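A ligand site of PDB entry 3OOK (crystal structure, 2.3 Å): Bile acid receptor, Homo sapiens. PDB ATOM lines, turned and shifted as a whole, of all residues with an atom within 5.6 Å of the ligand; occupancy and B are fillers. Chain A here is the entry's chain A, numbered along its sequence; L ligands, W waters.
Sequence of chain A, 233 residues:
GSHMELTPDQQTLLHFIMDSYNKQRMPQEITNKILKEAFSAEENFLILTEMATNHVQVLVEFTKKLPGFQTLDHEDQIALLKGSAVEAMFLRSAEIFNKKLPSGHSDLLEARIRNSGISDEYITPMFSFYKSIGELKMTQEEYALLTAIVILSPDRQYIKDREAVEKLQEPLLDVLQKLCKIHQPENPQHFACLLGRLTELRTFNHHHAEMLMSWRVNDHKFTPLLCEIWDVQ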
ATOM      1  N   GLN A  24     -19.406 -14.506  -7.346  1.00  0.00           N
ATOM      2  CA  GLN A  24     -20.480 -13.576  -7.045  1.00  0.00           C
ATOM      3  C   GLN A  24     -21.304 -13.138  -8.242  1.00  0.00           C
ATOM      4  O   GLN A  24     -20.793 -13.126  -9.360  1.00  0.00           O
ATOM      5  CB  GLN A  24     -19.872 -12.335  -6.376  1.00  0.00           C
ATOM      6  CG  GLN A  24     -20.832 -11.656  -5.438  1.00  0.00           C
ATOM      7  CD  GLN A  24     -20.561 -11.799  -3.963  1.00  0.00           C
ATOM      8  OE1 GLN A  24     -21.460 -11.656  -3.153  1.00  0.00           O
ATOM      9  NE2 GLN A  24     -19.325 -12.058  -3.590  1.00  0.00           N
ATOM     10  N   ARG A  25     -22.566 -12.714  -7.983  1.00  0.00           N
ATOM     11  CA  ARG A  25     -23.458 -12.159  -8.993  1.00  0.00           C
ATOM     12  C   ARG A  25     -22.818 -10.875  -9.567  1.00  0.00           C
ATOM     13  O   ARG A  25     -22.260 -10.084  -8.810  1.00  0.00           O
ATOM     14  CB  ARG A  25     -24.855 -11.883  -8.389  1.00  0.00           C
ATOM     15  CG  ARG A  25     -25.857 -11.303  -9.377  1.00  0.00           C
ATOM     16  CD  ARG A  25     -27.264 -11.322  -8.835  1.00  0.00           C
ATOM     17  NE  ARG A  25     -27.919 -12.602  -9.115  1.00  0.00           N
ATOM     18  CZ  ARG A  25     -29.220 -12.840  -8.958  1.00  0.00           C
ATOM     19  NH1 ARG A  25     -30.029 -11.887  -8.509  1.00  0.00           N
ATOM     20  NH2 ARG A  25     -29.727 -14.029  -9.249  1.00  0.00           N
ATOM     21  N   ILE A  30     -27.368  -5.881 -11.541  1.00  0.00           N
ATOM     22  CA  ILE A  30     -28.020  -5.194 -10.431  1.00  0.00           C
ATOM     23  C   ILE A  30     -28.267  -3.710 -10.722  1.00  0.00           C
ATOM     24  O   ILE A  30     -29.419  -3.268 -10.701  1.00  0.00           O
ATOM     25  CB  ILE A  30     -27.141  -5.434  -9.150  1.00  0.00           C
ATOM     26  CG1 ILE A  30     -26.839  -6.961  -8.972  1.00  0.00           C
ATOM     27  CG2 ILE A  30     -27.754  -4.785  -7.910  1.00  0.00           C
ATOM     28  CD1 ILE A  30     -25.612  -7.402  -8.220  1.00  0.00           C
ATOM     29  N   THR A  31     -27.174  -2.940 -10.982  1.00  0.00           N
ATOM     30  CA  THR A  31     -27.217  -1.506 -11.238  1.00  0.00           C
ATOM     31  C   THR A  31     -27.896  -1.060 -12.518  1.00  0.00           C
ATOM     32  O   THR A  31     -28.536  -0.010 -12.522  1.00  0.00           O
ATOM     33  CB  THR A  31     -25.866  -0.847 -11.036  1.00  0.00           C
ATOM     34  OG1 THR A  31     -24.926  -1.463 -11.894  1.00  0.00           O
ATOM     35  CG2 THR A  31     -25.431  -0.870  -9.583  1.00  0.00           C
ATOM     36  N   ILE A  34     -31.766  -1.355 -11.837  1.00  0.00           N
ATOM     37  CA  ILE A  34     -32.195  -0.231 -11.007  1.00  0.00           C
ATOM     38  C   ILE A  34     -32.198   1.069 -11.815  1.00  0.00           C
ATOM     39  O   ILE A  34     -33.154   1.820 -11.724  1.00  0.00           O
ATOM     40  CB  ILE A  34     -31.367  -0.129  -9.678  1.00  0.00           C
ATOM     41  CG1 ILE A  34     -31.543  -1.402  -8.803  1.00  0.00           C
ATOM     42  CG2 ILE A  34     -31.750   1.144  -8.869  1.00  0.00           C
ATOM     43  CD1 ILE A  34     -30.504  -1.588  -7.672  1.00  0.00           C
ATOM     44  N   ASN A  44     -39.911  -3.454  -6.538  1.00  0.00           N
ATOM     45  CA  ASN A  44     -38.646  -3.336  -5.853  1.00  0.00           C
ATOM     46  C   ASN A  44     -38.555  -4.269  -4.680  1.00  0.00           C
ATOM     47  O   ASN A  44     -37.486  -4.785  -4.429  1.00  0.00           O
ATOM     48  CB  ASN A  44     -38.392  -1.898  -5.445  1.00  0.00           C
ATOM     49  CG  ASN A  44     -37.950  -1.058  -6.608  1.00  0.00           C
ATOM     50  OD1 ASN A  44     -37.074  -1.446  -7.381  1.00  0.00           O
ATOM     51  ND2 ASN A  44     -38.533   0.116  -6.771  1.00  0.00           N
ATOM     52  N   ILE A  47     -37.761  -7.639  -6.264  1.00  0.00           N
ATOM     53  CA  ILE A  47     -36.370  -7.629  -6.714  1.00  0.00           C
ATOM     54  C   ILE A  47     -35.478  -7.844  -5.488  1.00  0.00           C
ATOM     55  O   ILE A  47     -34.590  -8.677  -5.521  1.00  0.00           O
ATOM     56  CB  ILE A  47     -36.007  -6.301  -7.484  1.00  0.00           C
ATOM     57  CG1 ILE A  47     -36.721  -6.267  -8.853  1.00  0.00           C
ATOM     58  CG2 ILE A  47     -34.461  -6.191  -7.667  1.00  0.00           C
ATOM     59  CD1 ILE A  47     -36.862  -4.844  -9.484  1.00  0.00           C
ATOM     60  N   LEU A  48     -35.760  -7.123  -4.404  1.00  0.00           N
ATOM     61  CA  LEU A  48     -35.011  -7.259  -3.155  1.00  0.00           C
ATOM     62  C   LEU A  48     -35.060  -8.695  -2.632  1.00  0.00           C
ATOM     63  O   LEU A  48     -33.994  -9.264  -2.343  1.00  0.00           O
ATOM     64  CB  LEU A  48     -35.464  -6.251  -2.082  1.00  0.00           C
ATOM     65  CG  LEU A  48     -35.009  -6.499  -0.605  1.00  0.00           C
ATOM     66  CD1 LEU A  48     -33.509  -6.303  -0.434  1.00  0.00           C
ATOM     67  CD2 LEU A  48     -35.777  -5.624   0.339  1.00  0.00           C
ATOM     68  N   MET A  51     -32.981 -10.953  -4.964  1.00  0.00           N
ATOM     69  CA  MET A  51     -31.562 -10.641  -4.876  1.00  0.00           C
ATOM     70  C   MET A  51     -31.012 -11.144  -3.539  1.00  0.00           C
ATOM     71  O   MET A  51     -29.923 -11.718  -3.501  1.00  0.00           O
ATOM     72  CB  MET A  51     -31.336  -9.122  -4.992  1.00  0.00           C
ATOM     73  CG  MET A  51     -31.531  -8.558  -6.408  1.00  0.00           C
ATOM     74  SD  MET A  51     -30.155  -8.959  -7.510  1.00  0.00           S
ATOM     75  CE  MET A  51     -28.787  -8.267  -6.614  1.00  0.00           C
ATOM     76  N   ALA A  52     -31.780 -10.961  -2.445  1.00  0.00           N
ATOM     77  CA  ALA A  52     -31.405 -11.353  -1.074  1.00  0.00           C
ATOM     78  C   ALA A  52     -31.414 -12.878  -0.869  1.00  0.00           C
ATOM     79  O   ALA A  52     -30.555 -13.389  -0.145  1.00  0.00           O
ATOM     80  CB  ALA A  52     -32.288 -10.661  -0.039  1.00  0.00           C
ATOM     81  N   ASN A  54     -30.837 -15.080  -3.379  1.00  0.00           N
ATOM     82  CA  ASN A  54     -29.690 -15.539  -4.164  1.00  0.00           C
ATOM     83  C   ASN A  54     -28.414 -15.218  -3.407  1.00  0.00           C
ATOM     84  O   ASN A  54     -27.481 -16.034  -3.439  1.00  0.00           O
ATOM     85  CB  ASN A  54     -29.651 -14.893  -5.567  1.00  0.00           C
ATOM     86  CG  ASN A  54     -28.354 -15.177  -6.304  1.00  0.00           C
ATOM     87  OD1 ASN A  54     -27.488 -14.287  -6.482  1.00  0.00           O
ATOM     88  ND2 ASN A  54     -28.137 -16.437  -6.655  1.00  0.00           N
ATOM     89  N   HIS A  55     -28.384 -14.046  -2.698  1.00  0.00           N
ATOM     90  CA  HIS A  55     -27.214 -13.627  -1.939  1.00  0.00           C
ATOM     91  C   HIS A  55     -26.884 -14.628  -0.863  1.00  0.00           C
ATOM     92  O   HIS A  55     -25.711 -14.986  -0.740  1.00  0.00           O
ATOM     93  CB  HIS A  55     -27.365 -12.217  -1.346  1.00  0.00           C
ATOM     94  CG  HIS A  55     -26.099 -11.760  -0.715  1.00  0.00           C
ATOM     95  ND1 HIS A  55     -25.828 -11.997   0.607  1.00  0.00           N
ATOM     96  CD2 HIS A  55     -25.015 -11.187  -1.288  1.00  0.00           C
ATOM     97  CE1 HIS A  55     -24.606 -11.541   0.820  1.00  0.00           C
ATOM     98  NE2 HIS A  55     -24.091 -11.006  -0.289  1.00  0.00           N
ATOM     99  N   MET A  89     -24.734  -8.970   3.225  1.00  0.00           N
ATOM    100  CA  MET A  89     -25.595  -8.444   2.174  1.00  0.00           C
ATOM    101  C   MET A  89     -25.438  -6.925   2.104  1.00  0.00           C
ATOM    102  O   MET A  89     -25.313  -6.390   1.006  1.00  0.00           O
ATOM    103  CB  MET A  89     -27.048  -8.882   2.430  1.00  0.00           C
ATOM    104  CG  MET A  89     -27.979  -8.659   1.248  1.00  0.00           C
ATOM    105  SD  MET A  89     -28.514  -6.923   1.083  1.00  0.00           S
ATOM    106  CE  MET A  89     -29.122  -6.634   2.652  1.00  0.00           C
ATOM    107  N   PHE A  90     -25.426  -6.237   3.279  1.00  0.00           N
ATOM    108  CA  PHE A  90     -25.203  -4.789   3.347  1.00  0.00           C
ATOM    109  C   PHE A  90     -23.808  -4.416   2.902  1.00  0.00           C
ATOM    110  O   PHE A  90     -23.636  -3.371   2.272  1.00  0.00           O
ATOM    111  CB  PHE A  90     -25.577  -4.175   4.736  1.00  0.00           C
ATOM    112  CG  PHE A  90     -27.071  -3.999   4.842  1.00  0.00           C
ATOM    113  CD1 PHE A  90     -27.726  -3.017   4.091  1.00  0.00           C
ATOM    114  CD2 PHE A  90     -27.840  -4.860   5.611  1.00  0.00           C
ATOM    115  CE1 PHE A  90     -29.115  -2.902   4.128  1.00  0.00           C
ATOM    116  CE2 PHE A  90     -29.233  -4.727   5.672  1.00  0.00           C
ATOM    117  CZ  PHE A  90     -29.867  -3.746   4.913  1.00  0.00           C
ATOM    118  N   ARG A  92     -21.966  -6.190   0.642  1.00  0.00           N
ATOM    119  CA  ARG A  92     -22.040  -6.389  -0.802  1.00  0.00           C
ATOM    120  C   ARG A  92     -22.833  -5.215  -1.454  1.00  0.00           C
ATOM    121  O   ARG A  92     -22.416  -4.722  -2.477  1.00  0.00           O
ATOM    122  CB  ARG A  92     -22.710  -7.755  -1.113  1.00  0.00           C
ATOM    123  CG  ARG A  92     -22.840  -8.095  -2.613  1.00  0.00           C
ATOM    124  CD  ARG A  92     -21.534  -8.043  -3.382  1.00  0.00           C
ATOM    125  NE  ARG A  92     -21.726  -8.429  -4.778  1.00  0.00           N
ATOM    126  CZ  ARG A  92     -20.758  -8.538  -5.673  1.00  0.00           C
ATOM    127  NH1 ARG A  92     -19.497  -8.321  -5.339  1.00  0.00           N
ATOM    128  NH2 ARG A  92     -21.035  -8.935  -6.917  1.00  0.00           N
ATOM    129  N   SER A  93     -23.941  -4.782  -0.837  1.00  0.00           N
ATOM    130  CA  SER A  93     -24.736  -3.645  -1.344  1.00  0.00           C
ATOM    131  C   SER A  93     -23.842  -2.393  -1.348  1.00  0.00           C
ATOM    132  O   SER A  93     -23.834  -1.679  -2.343  1.00  0.00           O
ATOM    133  CB  SER A  93     -25.989  -3.417  -0.502  1.00  0.00           C
ATOM    134  OG  SER A  93     -26.911  -4.481  -0.626  1.00  0.00           O
ATOM    135  N   ALA A  94     -23.033  -2.181  -0.276  1.00  0.00           N
ATOM    136  CA  ALA A  94     -22.078  -1.072  -0.120  1.00  0.00           C
ATOM    137  C   ALA A  94     -21.035  -1.085  -1.214  1.00  0.00           C
ATOM    138  O   ALA A  94     -20.768  -0.044  -1.784  1.00  0.00           O
ATOM    139  CB  ALA A  94     -21.408  -1.114   1.249  1.00  0.00           C
ATOM    140  N   ILE A  96     -21.243  -2.613  -4.333  1.00  0.00           N
ATOM    141  CA  ILE A  96     -21.944  -2.301  -5.571  1.00  0.00           C
ATOM    142  C   ILE A  96     -22.339  -0.836  -5.674  1.00  0.00           C
ATOM    143  O   ILE A  96     -22.326  -0.283  -6.766  1.00  0.00           O
ATOM    144  CB  ILE A  96     -23.121  -3.283  -5.803  1.00  0.00           C
ATOM    145  CG1 ILE A  96     -22.569  -4.681  -6.056  1.00  0.00           C
ATOM    146  CG2 ILE A  96     -23.987  -2.843  -6.984  1.00  0.00           C
ATOM    147  CD1 ILE A  96     -23.490  -5.703  -5.826  1.00  0.00           C
ATOM    148  N   PHE A  97     -22.660  -0.197  -4.548  1.00  0.00           N
ATOM    149  CA  PHE A  97     -23.039   1.201  -4.516  1.00  0.00           C
ATOM    150  C   PHE A  97     -21.855   2.087  -4.972  1.00  0.00           C
ATOM    151  O   PHE A  97     -22.071   3.053  -5.715  1.00  0.00           O
ATOM    152  CB  PHE A  97     -23.520   1.600  -3.111  1.00  0.00           C
ATOM    153  CG  PHE A  97     -24.058   3.001  -2.993  1.00  0.00           C
ATOM    154  CD1 PHE A  97     -25.356   3.301  -3.409  1.00  0.00           C
ATOM    155  CD2 PHE A  97     -23.274   4.034  -2.483  1.00  0.00           C
ATOM    156  CE1 PHE A  97     -25.858   4.609  -3.289  1.00  0.00           C
ATOM    157  CE2 PHE A  97     -23.784   5.332  -2.357  1.00  0.00           C
ATOM    158  CZ  PHE A  97     -25.076   5.608  -2.754  1.00  0.00           C
ATOM    159  N   ASN A  98     -20.632   1.721  -4.546  1.00  0.00           N
ATOM    160  CA  ASN A  98     -19.414   2.488  -4.868  1.00  0.00           C
ATOM    161  C   ASN A  98     -18.660   2.009  -6.094  1.00  0.00           C
ATOM    162  O   ASN A  98     -17.546   2.463  -6.347  1.00  0.00           O
ATOM    163  CB  ASN A  98     -18.515   2.657  -3.648  1.00  0.00           C
ATOM    164  CG  ASN A  98     -19.249   3.287  -2.520  1.00  0.00           C
ATOM    165  OD1 ASN A  98     -19.493   4.494  -2.494  1.00  0.00           O
ATOM    166  ND2 ASN A  98     -19.688   2.454  -1.598  1.00  0.00           N
ATOM    167  N   LEU A 109     -28.898   6.022  -9.210  1.00  0.00           N
ATOM    168  CA  LEU A 109     -28.931   4.764  -8.474  1.00  0.00           C
ATOM    169  C   LEU A 109     -29.317   5.068  -7.013  1.00  0.00           C
ATOM    170  O   LEU A 109     -30.211   4.404  -6.487  1.00  0.00           O
ATOM    171  CB  LEU A 109     -27.545   4.067  -8.549  1.00  0.00           C
ATOM    172  CG  LEU A 109     -27.302   2.804  -7.698  1.00  0.00           C
ATOM    173  CD1 LEU A 109     -28.064   1.603  -8.250  1.00  0.00           C
ATOM    174  CD2 LEU A 109     -25.834   2.461  -7.643  1.00  0.00           C
ATOM    175  N   ARG A 112     -33.038   6.249  -6.926  1.00  0.00           N
ATOM    176  CA  ARG A 112     -33.881   5.080  -7.157  1.00  0.00           C
ATOM    177  C   ARG A 112     -33.954   4.182  -5.917  1.00  0.00           C
ATOM    178  O   ARG A 112     -35.043   3.706  -5.575  1.00  0.00           O
ATOM    179  CB  ARG A 112     -33.398   4.287  -8.372  1.00  0.00           C
ATOM    180  CG  ARG A 112     -33.576   5.012  -9.700  1.00  0.00           C
ATOM    181  CD  ARG A 112     -34.943   4.814 -10.318  1.00  0.00           C
ATOM    182  NE  ARG A 112     -34.794   4.442 -11.727  1.00  0.00           N
ATOM    183  CZ  ARG A 112     -34.748   5.296 -12.737  1.00  0.00           C
ATOM    184  NH1 ARG A 112     -34.868   6.603 -12.512  1.00  0.00           N
ATOM    185  NH2 ARG A 112     -34.572   4.873 -13.974  1.00  0.00           N
ATOM    186  N   ILE A 113     -32.809   3.994  -5.204  1.00  0.00           N
ATOM    187  CA  ILE A 113     -32.798   3.192  -3.977  1.00  0.00           C
ATOM    188  C   ILE A 113     -33.560   3.951  -2.897  1.00  0.00           C
ATOM    189  O   ILE A 113     -34.368   3.371  -2.180  1.00  0.00           O
ATOM    190  CB  ILE A 113     -31.377   2.709  -3.537  1.00  0.00           C
ATOM    191  CG1 ILE A 113     -30.776   1.770  -4.610  1.00  0.00           C
ATOM    192  CG2 ILE A 113     -31.422   1.986  -2.157  1.00  0.00           C
ATOM    193  CD1 ILE A 113     -29.295   1.710  -4.573  1.00  0.00           C
ATOM    194  N   SER A 116     -37.221   3.403  -3.457  1.00  0.00           N
ATOM    195  CA  SER A 116     -37.487   1.990  -3.726  1.00  0.00           C
ATOM    196  C   SER A 116     -38.676   1.403  -2.951  1.00  0.00           C
ATOM    197  O   SER A 116     -39.233   0.417  -3.402  1.00  0.00           O
ATOM    198  CB  SER A 116     -36.249   1.145  -3.441  1.00  0.00           C
ATOM    199  OG  SER A 116     -35.841   1.317  -2.085  1.00  0.00           O
ATOM    200  N   ILE A 118     -38.335   1.334   0.745  1.00  0.00           N
ATOM    201  CA  ILE A 118     -37.747   1.251   2.092  1.00  0.00           C
ATOM    202  C   ILE A 118     -38.298   2.431   2.947  1.00  0.00           C
ATOM    203  O   ILE A 118     -38.493   3.534   2.418  1.00  0.00           O
ATOM    204  CB  ILE A 118     -36.183   1.237   2.016  1.00  0.00           C
ATOM    205  CG1 ILE A 118     -35.538   1.114   3.413  1.00  0.00           C
ATOM    206  CG2 ILE A 118     -35.613   2.422   1.199  1.00  0.00           C
ATOM    207  CD1 ILE A 118     -34.162   0.473   3.481  1.00  0.00           C
ATOM    208  N   MET A 126     -28.301   3.789   6.303  1.00  0.00           N
ATOM    209  CA  MET A 126     -27.918   2.911   5.197  1.00  0.00           C
ATOM    210  C   MET A 126     -27.009   3.627   4.185  1.00  0.00           C
ATOM    211  O   MET A 126     -25.975   3.071   3.821  1.00  0.00           O
ATOM    212  CB  MET A 126     -29.185   2.357   4.534  1.00  0.00           C
ATOM    213  CG  MET A 126     -28.924   1.334   3.460  1.00  0.00           C
ATOM    214  SD  MET A 126     -30.404   0.991   2.501  1.00  0.00           S
ATOM    215  CE  MET A 126     -30.327   2.261   1.360  1.00  0.00           C
ATOM    216  N   TYR A 130     -22.883   3.414   3.257  1.00  0.00           N
ATOM    217  CA  TYR A 130     -22.465   3.210   1.869  1.00  0.00           C
ATOM    218  C   TYR A 130     -21.410   4.241   1.463  1.00  0.00           C
ATOM    219  O   TYR A 130     -20.448   3.910   0.758  1.00  0.00           O
ATOM    220  CB  TYR A 130     -23.687   3.280   0.919  1.00  0.00           C
ATOM    221  CG  TYR A 130     -24.669   2.128   0.994  1.00  0.00           C
ATOM    222  CD1 TYR A 130     -24.412   1.012   1.783  1.00  0.00           C
ATOM    223  CD2 TYR A 130     -25.881   2.180   0.283  1.00  0.00           C
ATOM    224  CE1 TYR A 130     -25.336  -0.036   1.875  1.00  0.00           C
ATOM    225  CE2 TYR A 130     -26.792   1.125   0.345  1.00  0.00           C
ATOM    226  CZ  TYR A 130     -26.513   0.017   1.141  1.00  0.00           C
ATOM    227  OH  TYR A 130     -27.423  -1.019   1.206  1.00  0.00           O
ATOM    228  N   MET A 211     -36.870  -3.637   8.574  1.00  0.00           N
ATOM    229  CA  MET A 211     -36.508  -3.029   7.288  1.00  0.00           C
ATOM    230  C   MET A 211     -37.356  -3.660   6.192  1.00  0.00           C
ATOM    231  O   MET A 211     -37.807  -2.969   5.278  1.00  0.00           O
ATOM    232  CB  MET A 211     -35.031  -3.271   6.962  1.00  0.00           C
ATOM    233  CG  MET A 211     -34.238  -2.011   6.771  1.00  0.00           C
ATOM    234  SD  MET A 211     -32.453  -2.287   6.806  1.00  0.00           S
ATOM    235  CE  MET A 211     -32.274  -3.146   8.346  1.00  0.00           C
ATOM    236  N   LEU A 212     -37.547  -4.978   6.293  1.00  0.00           N
ATOM    237  CA  LEU A 212     -38.366  -5.717   5.340  1.00  0.00           C
ATOM    238  C   LEU A 212     -39.841  -5.513   5.641  1.00  0.00           C
ATOM    239  O   LEU A 212     -40.566  -5.173   4.720  1.00  0.00           O
ATOM    240  CB  LEU A 212     -37.989  -7.213   5.276  1.00  0.00           C
ATOM    241  CG  LEU A 212     -36.504  -7.583   5.006  1.00  0.00           C
ATOM    242  CD1 LEU A 212     -36.363  -9.063   4.605  1.00  0.00           C
ATOM    243  CD2 LEU A 212     -35.879  -6.704   3.904  1.00  0.00           C
ATOM    244  N   TRP A 215     -41.388  -2.124   4.559  1.00  0.00           N
ATOM    245  CA  TRP A 215     -41.348  -1.839   3.129  1.00  0.00           C
ATOM    246  C   TRP A 215     -42.767  -1.430   2.717  1.00  0.00           C
ATOM    247  O   TRP A 215     -43.743  -2.075   3.142  1.00  0.00           O
ATOM    248  CB  TRP A 215     -40.818  -3.030   2.295  1.00  0.00           C
ATOM    249  CG  TRP A 215     -40.246  -2.616   0.964  1.00  0.00           C
ATOM    250  CD1 TRP A 215     -40.934  -2.307  -0.168  1.00  0.00           C
ATOM    251  CD2 TRP A 215     -38.860  -2.379   0.654  1.00  0.00           C
ATOM    252  NE1 TRP A 215     -40.073  -1.950  -1.183  1.00  0.00           N
ATOM    253  CE2 TRP A 215     -38.786  -1.973  -0.700  1.00  0.00           C
ATOM    254  CE3 TRP A 215     -37.657  -2.464   1.397  1.00  0.00           C
ATOM    255  CZ2 TRP A 215     -37.576  -1.675  -1.345  1.00  0.00           C
ATOM    256  CZ3 TRP A 215     -36.454  -2.176   0.758  1.00  0.00           C
ATOM    257  CH2 TRP A 215     -36.424  -1.778  -0.594  1.00  0.00           C
ATOM    258  N   TRP A 230     -33.482 -13.892   7.731  1.00  0.00           N
ATOM    259  CA  TRP A 230     -34.011 -12.619   8.190  1.00  0.00           C
ATOM    260  C   TRP A 230     -35.025 -12.957   9.242  1.00  0.00           C
ATOM    261  O   TRP A 230     -35.490 -14.095   9.276  1.00  0.00           O
ATOM    262  CB  TRP A 230     -34.610 -11.826   7.009  1.00  0.00           C
ATOM    263  CG  TRP A 230     -33.565 -11.329   6.044  1.00  0.00           C
ATOM    264  CD1 TRP A 230     -32.827 -12.090   5.186  1.00  0.00           C
ATOM    265  CD2 TRP A 230     -33.077  -9.989   5.904  1.00  0.00           C
ATOM    266  NE1 TRP A 230     -31.939 -11.307   4.495  1.00  0.00           N
ATOM    267  CE2 TRP A 230     -32.079 -10.009   4.905  1.00  0.00           C
ATOM    268  CE3 TRP A 230     -33.381  -8.764   6.540  1.00  0.00           C
ATOM    269  CZ2 TRP A 230     -31.412  -8.845   4.488  1.00  0.00           C
ATOM    270  CZ3 TRP A 230     -32.743  -7.606   6.110  1.00  0.00           C
ATOM    271  CH2 TRP A 230     -31.762  -7.664   5.106  1.00  0.00           C
HETATM  272  N1  LIG L   1     -29.829  -2.923  -2.432  1.00  0.00           N
HETATM  273  C1  LIG L   1     -29.738  -2.371  -1.177  1.00  0.00           C
HETATM  274  N2  LIG L   1     -28.818  -1.447  -1.155  1.00  0.00           N
HETATM  275  C2  LIG L   1     -28.872  -2.308  -3.201  1.00  0.00           C
HETATM  276  C3  LIG L   1     -28.242  -1.359  -2.373  1.00  0.00           C
HETATM  277  C4  LIG L   1     -29.990  -5.125  -3.394  1.00  0.00           C
HETATM  278  N3  LIG L   1     -28.874  -5.490  -2.714  1.00  0.00           N
HETATM  279  C5  LIG L   1     -28.055  -6.541  -3.103  1.00  0.00           C
HETATM  280  C6  LIG L   1     -30.779  -3.949  -2.878  1.00  0.00           C
HETATM  281  C7  LIG L   1     -28.497  -2.454  -4.530  1.00  0.00           C
HETATM  282  C8  LIG L   1     -28.376  -7.864  -2.769  1.00  0.00           C
HETATM  283  C9  LIG L   1     -26.925  -6.259  -3.903  1.00  0.00           C
HETATM  284  C10 LIG L   1     -26.412  -8.602  -3.984  1.00  0.00           C
HETATM  285  C11 LIG L   1     -27.183  -0.601  -2.867  1.00  0.00           C
HETATM  286  C12 LIG L   1     -25.545  -9.694  -4.494  1.00  0.00           C
HETATM  287  C13 LIG L   1     -27.491  -1.662  -5.018  1.00  0.00           C
HETATM  288  C14 LIG L   1     -30.608  -2.729  -0.047  1.00  0.00           C
HETATM  289  C15 LIG L   1     -26.829  -0.766  -4.190  1.00  0.00           C
HETATM  290  C16 LIG L   1     -26.113  -7.286  -4.325  1.00  0.00           C
HETATM  291  C17 LIG L   1     -27.558  -8.889  -3.212  1.00  0.00           C
HETATM  292  O1  LIG L   1     -30.348  -5.736  -4.380  1.00  0.00           O
HETATM  293  O2  LIG L   1     -24.516  -9.467  -5.089  1.00  0.00           O
HETATM  294  C18 LIG L   1     -31.784  -3.308  -3.866  1.00  0.00           C
HETATM  295  C19 LIG L   1     -30.603  -4.041   0.409  1.00  0.00           C
HETATM  296  C20 LIG L   1     -31.514  -1.787   0.476  1.00  0.00           C
HETATM  297  F1  LIG L   1     -26.640  -4.999  -4.286  1.00  0.00           F
HETATM  298  F2  LIG L   1     -29.472  -8.132  -2.018  1.00  0.00           F
HETATM  299  F3  LIG L   1     -27.127  -1.791  -6.316  1.00  0.00           F
HETATM  300  F4  LIG L   1     -25.896   0.036  -4.717  1.00  0.00           F
HETATM  301  O3  LIG L   1     -25.928 -10.962  -4.336  1.00  0.00           O
HETATM  302  C21 LIG L   1     -32.296  -3.457   2.001  1.00  0.00           C
HETATM  303  C22 LIG L   1     -32.324  -2.151   1.523  1.00  0.00           C
HETATM  304  C23 LIG L   1     -31.427  -4.393   1.445  1.00  0.00           C
HETATM  305 CL1  LIG L   1     -33.325  -3.972   3.291  1.00  0.00          CL
HETATM  306  C24 LIG L   1     -32.997  -4.242  -4.047  1.00  0.00           C
HETATM  307  C25 LIG L   1     -32.245  -1.926  -3.341  1.00  0.00           C
HETATM  308  C26 LIG L   1     -34.061  -3.594  -4.954  1.00  0.00           C
HETATM  309  C27 LIG L   1     -33.241  -1.266  -4.320  1.00  0.00           C
HETATM  310  C28 LIG L   1     -34.472  -2.196  -4.436  1.00  0.00           C
HETATM  311  O   HOH W   1     -27.938 -11.932  -5.463  1.00  0.00           O
HETATM  312  O   HOH W   2     -23.874 -12.296  -4.596  1.00  0.00           O
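A nitrogen (N2) of the ligand is in hydrogen-bond range of the side-chain hydroxyl of Tyr 130, at 2.8 Å. NE of Arg 92 lies within salt-bridge range of O2 of the ligand (3.0 Å). A nitrogen (N3) of the ligand is in hydrogen-bond range of the side-chain hydroxyl (OG) of Ser 93.
The backbone carbonyl oxygen of Tyr 130 sits at hydrogen-bond distance from the side-chain amide nitrogen of Asn 98 (2.9 Å). NH2 of Arg 92 sits at hydrogen-bond distance from O of Arg 25 (2.5 Å). OG of Ser 93 lies within hydrogen-bond range of O of Met 89 (3.0 Å). The backbone carbonyl oxygen (O) of Ile 113 is in hydrogen-bond range of the side-chain hydroxyl (OG) of Ser 116 (2.5 Å). The guanidinium group (NH1) of Arg 25 is in hydrogen-bond range of the side-chain sulfur (SD) of Met 51, at 3.1 Å. O of Ile 34 lies within hydrogen-bond range of NE of Arg 112 (3.1 Å). ND2 of Asn 44 lies close to O of Ser 116. O of Ser 116 sits at hydrogen-bond distance from NE1 of Trp 215 (3.4 Å).
SD of Met 89 sits close to F2 of the ligand, at 3.5 Å. F4 of the ligand sits close to N of Phe 97 (3.2 Å). Residues that only touch the ligand: Ile 30, Thr 31, Ile 34, Asn 44, Ile 47, Leu 48, Met 51, Ala 52, His 55, Phe 90, Ile 96, Leu 109, Ile 113, Ser 116, Ile 118, Met 126, Met 211 and Leu 212. Hydrophobic or aromatic side chains within 4 Å of the ligand: Ile 30, Ile 34, Ile 47, Leu 48, Met 51, His 55, Met 89, Phe 90, Ile 96, Phe 97, Leu 109, Ile 113, Ile 118, Met 126, Tyr 130, Met 211 and Leu 212. Of the 31 residues printed, 23 come within 4 Å of the ligand. The nearest printed residue that does not touch the ligand is Arg 25 (4.1 Å).
Water W2 bridges O3 of the ligand (2.5 Å) and OE1 of Gln 24 (2.9 Å). Water W1 lies within hydrogen-bond range of O3 of the ligand, OD1 of Asn 54 and O of Met 51.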
